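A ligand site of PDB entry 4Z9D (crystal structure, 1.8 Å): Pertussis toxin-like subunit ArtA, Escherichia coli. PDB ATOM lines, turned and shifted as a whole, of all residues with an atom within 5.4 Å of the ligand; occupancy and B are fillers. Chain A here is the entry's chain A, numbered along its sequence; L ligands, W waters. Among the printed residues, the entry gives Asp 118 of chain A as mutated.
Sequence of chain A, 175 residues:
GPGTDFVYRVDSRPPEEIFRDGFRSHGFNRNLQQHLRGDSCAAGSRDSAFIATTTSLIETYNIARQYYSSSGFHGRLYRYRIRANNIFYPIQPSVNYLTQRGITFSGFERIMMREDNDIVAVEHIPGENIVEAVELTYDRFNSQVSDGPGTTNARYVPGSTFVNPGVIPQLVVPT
The backbone NH (N) of Ser 12 lies within hydrogen-bond range of an oxygen (O5) of the ligand (3.2 Å).
The side-chain hydroxyl (OG) of Ser 12 sits at hydrogen-bond distance from an oxygen (O6) of the ligand (2.5 Å).
NH1 of Arg 9 is in salt-bridge range of O8 of the ligand (2.5 Å).
An oxygen (O9) of the ligand is in hydrogen-bond range of the side-chain hydroxyl (OH) of Tyr 67, 2.7 Å away.
A ring nitrogen (NE2) of His 26 sits at hydrogen-bond distance from an oxygen (O2) of the ligand (2.7 Å).
The backbone carbonyl oxygen of Arg 24 lies within hydrogen-bond range of a nitrogen (N3) of the ligand, at 2.8 Å.
The backbone NH (N) of Val 10 lies within hydrogen-bond range of an oxygen (O14) of the ligand.
The backbone carbonyl oxygen (O) of Val 10 is in hydrogen-bond range of a nitrogen (N7) of the ligand, 3.2 Å away.
O2 of the ligand lies within hydrogen-bond range of N of Ala 42.
O of Leu 36 lies within hydrogen-bond range of O12 of the ligand (3.1 Å).
O12 of the ligand sits at hydrogen-bond distance from O of His 35 (3.3 Å).
OD1 of Asp 11 is in hydrogen-bond range of O5 of the ligand (3.3 Å).
Water W6 bridges the backbone carbonyl oxygen of Val 10 (2.8 Å) and an oxygen (O5) of the ligand (2.8 Å).
Water W1 bridges O of Leu 36 (2.5 Å) and O12 of the ligand (2.9 Å).
Water W7 lies within hydrogen-bond range of N of Ala 52 (2.8 Å) and O8 of the ligand (2.9 Å).
Water W4 bridges the backbone carbonyl oxygen of Ser 25 and a nitrogen (N3) of the ligand.
Water W5 lies within hydrogen-bond range of O of Arg 24, NH2 of Arg 13 and N2 of the ligand.
NH2 of Arg 13 touches C6 of the ligand, at 3.5 Å.
Ser 25 touches the ligand (O to N3, 3.6 Å).
Gly 38 touches the ligand (N to O12, 3.7 Å).
Cys 41 touches the ligand (CB to O2, 3.6 Å).
Ala 52 touches the ligand (CB to C16, 3.6 Å).
Thr 53 touches the ligand.
Ile 63 touches the ligand.
Asp 118 touches the ligand.
18 residues have an atom within 4 Å of the ligand: Arg 9, Val 10, Asp 11, Ser 12, Arg 13, Arg 24, Ser 25, His 26, His 35, Leu 36, Gly 38, Cys 41, Ala 42, Ala 52, Thr 53, Ile 63, Tyr 67 and Asp 118.
The guanidinium group (NH2) of Arg 9 is in salt-bridge range of the side-chain carboxylate (OD2) of Asp 11, 2.9 Å away.
NH1 of Arg 9 is in hydrogen-bond range of O of Ala 52 (3.0 Å).
O of Ala 42 is in hydrogen-bond range of NE of Arg 46, at 2.5 Å.
A ring nitrogen (ND1) of His 35 sits at hydrogen-bond distance from the side-chain sulfur (SG) of Cys 41 (3.5 Å).
The guanidinium group of Arg 13 is in salt-bridge range of the side-chain carboxylate of Asp 11 (2.8 Å).
The backbone carbonyl oxygen of Cys 41 lies within hydrogen-bond range of the backbone NH of Arg 46, at 3.2 Å.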
ATOM      1  N   TYR A   8     -16.690 -15.710   8.049  1.00  0.00           N
ATOM      2  CA  TYR A   8     -17.357 -16.621   8.971  1.00  0.00           C
ATOM      3  C   TYR A   8     -18.661 -17.176   8.419  1.00  0.00           C
ATOM      4  O   TYR A   8     -19.373 -16.479   7.685  1.00  0.00           O
ATOM      5  CB  TYR A   8     -17.677 -15.946  10.286  1.00  0.00           C
ATOM      6  CG  TYR A   8     -16.505 -15.431  11.073  1.00  0.00           C
ATOM      7  CD1 TYR A   8     -15.733 -16.286  11.849  1.00  0.00           C
ATOM      8  CD2 TYR A   8     -16.201 -14.077  11.073  1.00  0.00           C
ATOM      9  CE1 TYR A   8     -14.682 -15.793  12.600  1.00  0.00           C
ATOM     10  CE2 TYR A   8     -15.141 -13.588  11.813  1.00  0.00           C
ATOM     11  CZ  TYR A   8     -14.382 -14.454  12.584  1.00  0.00           C
ATOM     12  OH  TYR A   8     -13.341 -13.953  13.325  1.00  0.00           O
ATOM     13  N   ARG A   9     -19.018 -18.376   8.838  1.00  0.00           N
ATOM     14  CA  ARG A   9     -20.350 -18.904   8.556  1.00  0.00           C
ATOM     15  C   ARG A   9     -20.910 -19.614   9.773  1.00  0.00           C
ATOM     16  O   ARG A   9     -20.216 -20.415  10.392  1.00  0.00           O
ATOM     17  CB  ARG A   9     -20.331 -19.870   7.353  1.00  0.00           C
ATOM     18  CG  ARG A   9     -21.695 -20.552   7.108  1.00  0.00           C
ATOM     19  CD  ARG A   9     -21.804 -21.307   5.776  1.00  0.00           C
ATOM     20  NE  ARG A   9     -23.044 -22.090   5.757  1.00  0.00           N
ATOM     21  CZ  ARG A   9     -24.248 -21.608   5.506  1.00  0.00           C
ATOM     22  NH1 ARG A   9     -24.396 -20.324   5.185  1.00  0.00           N
ATOM     23  NH2 ARG A   9     -25.307 -22.405   5.553  1.00  0.00           N
ATOM     24  N   VAL A  10     -22.142 -19.289  10.137  1.00  0.00           N
ATOM     25  CA  VAL A  10     -22.862 -20.008  11.175  1.00  0.00           C
ATOM     26  C   VAL A  10     -23.673 -21.133  10.530  1.00  0.00           C
ATOM     27  O   VAL A  10     -24.426 -20.888   9.590  1.00  0.00           O
ATOM     28  CB  VAL A  10     -23.777 -19.071  11.978  1.00  0.00           C
ATOM     29  CG1 VAL A  10     -24.528 -19.857  13.061  1.00  0.00           C
ATOM     30  CG2 VAL A  10     -22.949 -17.979  12.618  1.00  0.00           C
ATOM     31  N   ASP A  11     -23.504 -22.360  11.021  1.00  0.00           N
ATOM     32  CA  ASP A  11     -24.189 -23.529  10.440  1.00  0.00           C
ATOM     33  C   ASP A  11     -24.479 -24.565  11.529  1.00  0.00           C
ATOM     34  O   ASP A  11     -23.746 -24.672  12.509  1.00  0.00           O
ATOM     35  CB  ASP A  11     -23.326 -24.136   9.315  1.00  0.00           C
ATOM     36  CG  ASP A  11     -24.135 -24.990   8.344  1.00  0.00           C
ATOM     37  OD1 ASP A  11     -24.668 -26.041   8.766  1.00  0.00           O
ATOM     38  OD2 ASP A  11     -24.249 -24.612   7.148  1.00  0.00           O
ATOM     39  N   SER A  12     -25.523 -25.377  11.346  1.00  0.00           N
ATOM     40  CA  SER A  12     -25.885 -26.341  12.375  1.00  0.00           C
ATOM     41  C   SER A  12     -25.115 -27.658  12.257  1.00  0.00           C
ATOM     42  O   SER A  12     -25.097 -28.459  13.186  1.00  0.00           O
ATOM     43  CB  SER A  12     -27.382 -26.639  12.313  1.00  0.00           C
ATOM     44  OG  SER A  12     -27.757 -27.093  11.021  1.00  0.00           O
ATOM     45  N   ARG A  13     -24.487 -27.882  11.102  1.00  0.00           N
ATOM     46  CA  ARG A  13     -23.742 -29.112  10.881  1.00  0.00           C
ATOM     47  C   ARG A  13     -22.375 -29.058  11.558  1.00  0.00           C
ATOM     48  O   ARG A  13     -21.752 -28.005  11.604  1.00  0.00           O
ATOM     49  CB  ARG A  13     -23.589 -29.390   9.384  1.00  0.00           C
ATOM     50  CG  ARG A  13     -24.914 -29.757   8.752  1.00  0.00           C
ATOM     51  CD  ARG A  13     -24.902 -29.568   7.249  1.00  0.00           C
ATOM     52  NE  ARG A  13     -24.840 -28.183   6.821  1.00  0.00           N
ATOM     53  CZ  ARG A  13     -24.559 -27.837   5.574  1.00  0.00           C
ATOM     54  NH1 ARG A  13     -24.352 -28.801   4.683  1.00  0.00           N
ATOM     55  NH2 ARG A  13     -24.500 -26.550   5.205  1.00  0.00           N
ATOM     56  N   ARG A  24     -21.935 -26.919   0.631  1.00  0.00           N
ATOM     57  CA  ARG A  24     -22.480 -26.901  -0.727  1.00  0.00           C
ATOM     58  C   ARG A  24     -23.811 -26.153  -0.734  1.00  0.00           C
ATOM     59  O   ARG A  24     -24.600 -26.269   0.206  1.00  0.00           O
ATOM     60  CB  ARG A  24     -22.650 -28.326  -1.279  1.00  0.00           C
ATOM     61  CG  ARG A  24     -23.279 -28.382  -2.665  1.00  0.00           C
ATOM     62  CD  ARG A  24     -23.007 -29.712  -3.394  1.00  0.00           C
ATOM     63  NE  ARG A  24     -21.586 -29.962  -3.633  1.00  0.00           N
ATOM     64  CZ  ARG A  24     -20.874 -29.451  -4.634  1.00  0.00           C
ATOM     65  NH1 ARG A  24     -19.581 -29.759  -4.740  1.00  0.00           N
ATOM     66  NH2 ARG A  24     -21.411 -28.632  -5.517  1.00  0.00           N
ATOM     67  N   SER A  25     -24.064 -25.382  -1.790  1.00  0.00           N
ATOM     68  CA  SER A  25     -25.300 -24.598  -1.866  1.00  0.00           C
ATOM     69  C   SER A  25     -26.495 -25.527  -2.021  1.00  0.00           C
ATOM     70  O   SER A  25     -26.340 -26.704  -2.351  1.00  0.00           O
ATOM     71  CB  SER A  25     -25.275 -23.631  -3.046  1.00  0.00           C
ATOM     72  OG  SER A  25     -25.109 -24.344  -4.270  1.00  0.00           O
ATOM     73  N   HIS A  26     -27.690 -24.998  -1.772  1.00  0.00           N
ATOM     74  CA  HIS A  26     -28.924 -25.767  -1.964  1.00  0.00           C
ATOM     75  C   HIS A  26     -29.133 -26.138  -3.435  1.00  0.00           C
ATOM     76  O   HIS A  26     -29.550 -27.253  -3.763  1.00  0.00           O
ATOM     77  CB  HIS A  26     -30.138 -24.984  -1.486  1.00  0.00           C
ATOM     78  CG  HIS A  26     -30.193 -24.800  -0.002  1.00  0.00           C
ATOM     79  ND1 HIS A  26     -30.587 -25.814   0.847  1.00  0.00           N
ATOM     80  CD2 HIS A  26     -29.946 -23.723   0.777  1.00  0.00           C
ATOM     81  CE1 HIS A  26     -30.545 -25.370   2.097  1.00  0.00           C
ATOM     82  NE2 HIS A  26     -30.163 -24.110   2.077  1.00  0.00           N
ATOM     83  N   HIS A  35     -31.919 -14.717  -2.598  1.00  0.00           N
ATOM     84  CA  HIS A  35     -31.019 -15.268  -1.600  1.00  0.00           C
ATOM     85  C   HIS A  35     -30.886 -14.346  -0.370  1.00  0.00           C
ATOM     86  O   HIS A  35     -30.992 -14.798   0.770  1.00  0.00           O
ATOM     87  CB  HIS A  35     -29.652 -15.515  -2.208  1.00  0.00           C
ATOM     88  CG  HIS A  35     -28.616 -15.874  -1.193  1.00  0.00           C
ATOM     89  ND1 HIS A  35     -28.499 -17.150  -0.669  1.00  0.00           N
ATOM     90  CD2 HIS A  35     -27.676 -15.117  -0.567  1.00  0.00           C
ATOM     91  CE1 HIS A  35     -27.524 -17.164   0.222  1.00  0.00           C
ATOM     92  NE2 HIS A  35     -27.001 -15.951   0.295  1.00  0.00           N
ATOM     93  N   LEU A  36     -30.659 -13.061  -0.632  1.00  0.00           N
ATOM     94  CA  LEU A  36     -30.403 -12.109   0.442  1.00  0.00           C
ATOM     95  C   LEU A  36     -31.623 -11.960   1.366  1.00  0.00           C
ATOM     96  O   LEU A  36     -31.464 -11.674   2.564  1.00  0.00           O
ATOM     97  CB  LEU A  36     -29.991 -10.759  -0.133  1.00  0.00           C
ATOM     98  CG  LEU A  36     -28.653 -10.693  -0.894  1.00  0.00           C
ATOM     99  CD1 LEU A  36     -28.463  -9.310  -1.481  1.00  0.00           C
ATOM    100  CD2 LEU A  36     -27.498 -11.045   0.025  1.00  0.00           C
ATOM    101  N   ARG A  37     -32.825 -12.157   0.814  1.00  0.00           N
ATOM    102  CA  ARG A  37     -34.043 -12.131   1.634  1.00  0.00           C
ATOM    103  C   ARG A  37     -34.215 -13.396   2.459  1.00  0.00           C
ATOM    104  O   ARG A  37     -34.919 -13.385   3.465  1.00  0.00           O
ATOM    105  CB  ARG A  37     -35.284 -11.968   0.761  1.00  0.00           C
ATOM    106  CG  ARG A  37     -35.336 -10.709  -0.065  1.00  0.00           C
ATOM    107  CD  ARG A  37     -36.630 -10.743  -0.875  1.00  0.00           C
ATOM    108  NE  ARG A  37     -36.747  -9.636  -1.816  1.00  0.00           N
ATOM    109  CZ  ARG A  37     -36.949  -9.804  -3.122  1.00  0.00           C
ATOM    110  NH1 ARG A  37     -37.059 -11.032  -3.622  1.00  0.00           N
ATOM    111  NH2 ARG A  37     -37.054  -8.756  -3.933  1.00  0.00           N
ATOM    112  N   GLY A  38     -33.621 -14.483   2.005  1.00  0.00           N
ATOM    113  CA  GLY A  38     -33.803 -15.777   2.650  1.00  0.00           C
ATOM    114  C   GLY A  38     -34.811 -16.649   1.931  1.00  0.00           C
ATOM    115  O   GLY A  38     -35.035 -17.796   2.313  1.00  0.00           O
ATOM    116  N   CYS A  41     -33.384 -19.938   0.526  1.00  0.00           N
ATOM    117  CA  CYS A  41     -32.579 -20.709   1.463  1.00  0.00           C
ATOM    118  C   CYS A  41     -33.455 -21.708   2.205  1.00  0.00           C
ATOM    119  O   CYS A  41     -34.574 -22.018   1.753  1.00  0.00           O
ATOM    120  CB  CYS A  41     -31.862 -19.785   2.441  1.00  0.00           C
ATOM    121  SG  CYS A  41     -30.589 -18.781   1.627  1.00  0.00           S
ATOM    122  N   ALA A  42     -32.977 -22.203   3.336  1.00  0.00           N
ATOM    123  CA  ALA A  42     -33.622 -23.329   4.018  1.00  0.00           C
ATOM    124  C   ALA A  42     -35.091 -23.080   4.350  1.00  0.00           C
ATOM    125  O   ALA A  42     -35.905 -23.998   4.292  1.00  0.00           O
ATOM    126  CB  ALA A  42     -32.852 -23.670   5.287  1.00  0.00           C
ATOM    127  N   ALA A  43     -35.446 -21.844   4.657  1.00  0.00           N
ATOM    128  CA  ALA A  43     -36.835 -21.551   5.016  1.00  0.00           C
ATOM    129  C   ALA A  43     -37.695 -21.253   3.795  1.00  0.00           C
ATOM    130  O   ALA A  43     -38.880 -20.943   3.934  1.00  0.00           O
ATOM    131  CB  ALA A  43     -36.887 -20.389   5.983  1.00  0.00           C
ATOM    132  N   ARG A  46     -35.289 -23.306  -1.135  1.00  0.00           N
ATOM    133  CA  ARG A  46     -34.162 -24.232  -0.928  1.00  0.00           C
ATOM    134  C   ARG A  46     -33.460 -24.597  -2.227  1.00  0.00           C
ATOM    135  O   ARG A  46     -33.218 -25.779  -2.518  1.00  0.00           O
ATOM    136  CB  ARG A  46     -34.659 -25.501  -0.234  1.00  0.00           C
ATOM    137  CG  ARG A  46     -35.444 -25.202   1.034  1.00  0.00           C
ATOM    138  CD  ARG A  46     -35.898 -26.460   1.739  1.00  0.00           C
ATOM    139  NE  ARG A  46     -35.886 -26.279   3.191  1.00  0.00           N
ATOM    140  CZ  ARG A  46     -34.895 -26.664   3.991  1.00  0.00           C
ATOM    141  NH1 ARG A  46     -33.812 -27.243   3.502  1.00  0.00           N
ATOM    142  NH2 ARG A  46     -34.992 -26.445   5.295  1.00  0.00           N
ATOM    143  N   ALA A  52     -23.986 -18.342   2.200  1.00  0.00           N
ATOM    144  CA  ALA A  52     -23.822 -17.066   2.888  1.00  0.00           C
ATOM    145  C   ALA A  52     -22.680 -17.092   3.889  1.00  0.00           C
ATOM    146  O   ALA A  52     -22.514 -18.059   4.636  1.00  0.00           O
ATOM    147  CB  ALA A  52     -25.108 -16.690   3.604  1.00  0.00           C
ATOM    148  N   THR A  53     -21.903 -16.012   3.921  1.00  0.00           N
ATOM    149  CA  THR A  53     -20.856 -15.811   4.931  1.00  0.00           C
ATOM    150  C   THR A  53     -20.834 -14.343   5.339  1.00  0.00           C
ATOM    151  O   THR A  53     -21.517 -13.524   4.714  1.00  0.00           O
ATOM    152  CB  THR A  53     -19.440 -16.201   4.415  1.00  0.00           C
ATOM    153  OG1 THR A  53     -18.996 -15.234   3.454  1.00  0.00           O
ATOM    154  CG2 THR A  53     -19.427 -17.584   3.767  1.00  0.00           C
ATOM    155  N   THR A  54     -20.074 -14.009   6.375  1.00  0.00           N
ATOM    156  CA  THR A  54     -19.941 -12.608   6.760  1.00  0.00           C
ATOM    157  C   THR A  54     -18.520 -12.354   7.237  1.00  0.00           C
ATOM    158  O   THR A  54     -17.868 -13.255   7.785  1.00  0.00           O
ATOM    159  CB  THR A  54     -20.926 -12.213   7.912  1.00  0.00           C
ATOM    160  OG1 THR A  54     -20.683 -10.854   8.321  1.00  0.00           O
ATOM    161  CG2 THR A  54     -20.728 -13.127   9.112  1.00  0.00           C
ATOM    162  N   ILE A  63     -26.629 -13.473  14.233  1.00  0.00           N
ATOM    163  CA  ILE A  63     -27.218 -14.507  13.377  1.00  0.00           C
ATOM    164  C   ILE A  63     -27.533 -15.764  14.194  1.00  0.00           C
ATOM    165  O   ILE A  63     -28.623 -16.347  14.073  1.00  0.00           O
ATOM    166  CB  ILE A  63     -26.270 -14.852  12.208  1.00  0.00           C
ATOM    167  CG1 ILE A  63     -26.169 -13.664  11.238  1.00  0.00           C
ATOM    168  CG2 ILE A  63     -26.735 -16.103  11.462  1.00  0.00           C
ATOM    169  CD1 ILE A  63     -25.022 -13.801  10.230  1.00  0.00           C
ATOM    170  N   TYR A  67     -31.302 -17.658  15.106  1.00  0.00           N
ATOM    171  CA  TYR A  67     -31.622 -19.059  14.900  1.00  0.00           C
ATOM    172  C   TYR A  67     -31.964 -19.767  16.214  1.00  0.00           C
ATOM    173  O   TYR A  67     -32.941 -20.502  16.283  1.00  0.00           O
ATOM    174  CB  TYR A  67     -30.450 -19.763  14.209  1.00  0.00           C
ATOM    175  CG  TYR A  67     -30.192 -19.239  12.812  1.00  0.00           C
ATOM    176  CD1 TYR A  67     -31.125 -18.450  12.166  1.00  0.00           C
ATOM    177  CD2 TYR A  67     -29.007 -19.507  12.158  1.00  0.00           C
ATOM    178  CE1 TYR A  67     -30.901 -17.950  10.898  1.00  0.00           C
ATOM    179  CE2 TYR A  67     -28.764 -19.019  10.889  1.00  0.00           C
ATOM    180  CZ  TYR A  67     -29.716 -18.244  10.261  1.00  0.00           C
ATOM    181  OH  TYR A  67     -29.483 -17.754   8.994  1.00  0.00           O
ATOM    182  N   LEU A  77     -25.234 -24.907  17.054  1.00  0.00           N
ATOM    183  CA  LEU A  77     -24.737 -24.056  15.989  1.00  0.00           C
ATOM    184  C   LEU A  77     -23.244 -23.935  16.162  1.00  0.00           C
ATOM    185  O   LEU A  77     -22.734 -23.964  17.288  1.00  0.00           O
ATOM    186  CB  LEU A  77     -25.393 -22.679  16.017  1.00  0.00           C
ATOM    187  CG  LEU A  77     -26.868 -22.624  15.698  1.00  0.00           C
ATOM    188  CD1 LEU A  77     -27.381 -21.208  15.901  1.00  0.00           C
ATOM    189  CD2 LEU A  77     -27.051 -23.072  14.254  1.00  0.00           C
ATOM    190  N   ASP A 118     -21.511  -8.639   4.013  1.00  0.00           N
ATOM    191  CA  ASP A 118     -21.989  -9.855   3.355  1.00  0.00           C
ATOM    192  C   ASP A 118     -21.099 -10.276   2.195  1.00  0.00           C
ATOM    193  O   ASP A 118     -20.739  -9.462   1.333  1.00  0.00           O
ATOM    194  CB  ASP A 118     -23.420  -9.691   2.841  1.00  0.00           C
ATOM    195  CG  ASP A 118     -24.412  -9.502   3.965  1.00  0.00           C
ATOM    196  OD1 ASP A 118     -24.746 -10.526   4.607  1.00  0.00           O
ATOM    197  OD2 ASP A 118     -24.859  -8.353   4.197  1.00  0.00           O
HETATM  198  P1  LIG L   1     -28.928 -21.880   4.744  1.00  0.00           P
HETATM  199  O1  LIG L   1     -27.682 -21.853   3.935  1.00  0.00           O
HETATM  200  O2  LIG L   1     -30.175 -22.437   4.160  1.00  0.00           O
HETATM  201  O3  LIG L   1     -28.563 -22.647   6.137  1.00  0.00           O
HETATM  202  C1  LIG L   1     -29.524 -22.957   7.160  1.00  0.00           C
HETATM  203  C2  LIG L   1     -29.341 -24.449   7.530  1.00  0.00           C
HETATM  204  O4  LIG L   1     -29.745 -25.299   6.413  1.00  0.00           O
HETATM  205  C3  LIG L   1     -27.884 -24.750   7.709  1.00  0.00           C
HETATM  206  O5  LIG L   1     -27.493 -24.287   9.038  1.00  0.00           O
HETATM  207  C4  LIG L   1     -27.940 -26.245   7.639  1.00  0.00           C
HETATM  208  O6  LIG L   1     -28.680 -26.710   8.759  1.00  0.00           O
HETATM  209  C5  LIG L   1     -28.826 -26.430   6.397  1.00  0.00           C
HETATM  210  N1  LIG L   1     -28.184 -26.348   5.041  1.00  0.00           N
HETATM  211  C6  LIG L   1     -27.689 -25.337   4.321  1.00  0.00           C
HETATM  212  N2  LIG L   1     -27.289 -25.833   3.144  1.00  0.00           N
HETATM  213  C7  LIG L   1     -27.551 -27.143   3.124  1.00  0.00           C
HETATM  214  C8  LIG L   1     -27.349 -28.098   2.190  1.00  0.00           C
HETATM  215  N3  LIG L   1     -26.793 -27.710   1.050  1.00  0.00           N
HETATM  216  N4  LIG L   1     -27.695 -29.380   2.399  1.00  0.00           N
HETATM  217  C9  LIG L   1     -28.276 -29.724   3.615  1.00  0.00           C
HETATM  218  N5  LIG L   1     -28.479 -28.712   4.565  1.00  0.00           N
HETATM  219  C10 LIG L   1     -28.113 -27.449   4.296  1.00  0.00           C
HETATM  220  O7  LIG L   1     -29.260 -20.416   5.237  1.00  0.00           O
HETATM  221  P2  LIG L   1     -28.148 -19.408   5.870  1.00  0.00           P
HETATM  222  O8  LIG L   1     -26.832 -19.593   5.212  1.00  0.00           O
HETATM  223  O9  LIG L   1     -28.268 -19.449   7.353  1.00  0.00           O
HETATM  224  O10 LIG L   1     -28.747 -18.042   5.324  1.00  0.00           O
HETATM  225  C11 LIG L   1     -30.098 -17.635   5.581  1.00  0.00           C
HETATM  226  C12 LIG L   1     -30.197 -16.107   5.544  1.00  0.00           C
HETATM  227  O11 LIG L   1     -29.135 -15.652   6.461  1.00  0.00           O
HETATM  228  C13 LIG L   1     -29.852 -15.546   4.153  1.00  0.00           C
HETATM  229  O12 LIG L   1     -30.494 -14.288   3.948  1.00  0.00           O
HETATM  230  C14 LIG L   1     -28.366 -15.318   4.331  1.00  0.00           C
HETATM  231  O13 LIG L   1     -27.858 -14.392   3.348  1.00  0.00           O
HETATM  232  C15 LIG L   1     -28.286 -14.749   5.739  1.00  0.00           C
HETATM  233  N6  LIG L   1     -26.858 -14.815   6.227  1.00  0.00           N
HETATM  234  C16 LIG L   1     -26.384 -15.977   6.877  1.00  0.00           C
HETATM  235  C17 LIG L   1     -25.063 -16.104   7.306  1.00  0.00           C
HETATM  236  C18 LIG L   1     -24.598 -17.265   7.958  1.00  0.00           C
HETATM  237  O14 LIG L   1     -23.408 -17.191   8.587  1.00  0.00           O
HETATM  238  N7  LIG L   1     -25.378 -18.343   7.968  1.00  0.00           N
HETATM  239  C19 LIG L   1     -24.191 -15.028   7.091  1.00  0.00           C
HETATM  240  C20 LIG L   1     -24.653 -13.872   6.462  1.00  0.00           C
HETATM  241  C21 LIG L   1     -25.966 -13.748   6.021  1.00  0.00           C
HETATM  242  O   HOH W   1     -29.252 -11.669   3.828  1.00  0.00           O
HETATM  243  O   HOH W   2     -26.215 -23.344   2.195  1.00  0.00           O
HETATM  244  O   HOH W   3     -28.213 -32.659   4.744  1.00  0.00           O
HETATM  245  O   HOH W   4     -26.529 -29.525  -1.839  1.00  0.00           O
HETATM  246  O   HOH W   5     -23.947 -25.008   2.765  1.00  0.00           O
HETATM  247  O   HOH W   6     -26.978 -21.532   8.779  1.00  0.00           O
HETATM  248  O   HOH W   7     -26.505 -19.652   2.321  1.00  0.00           O
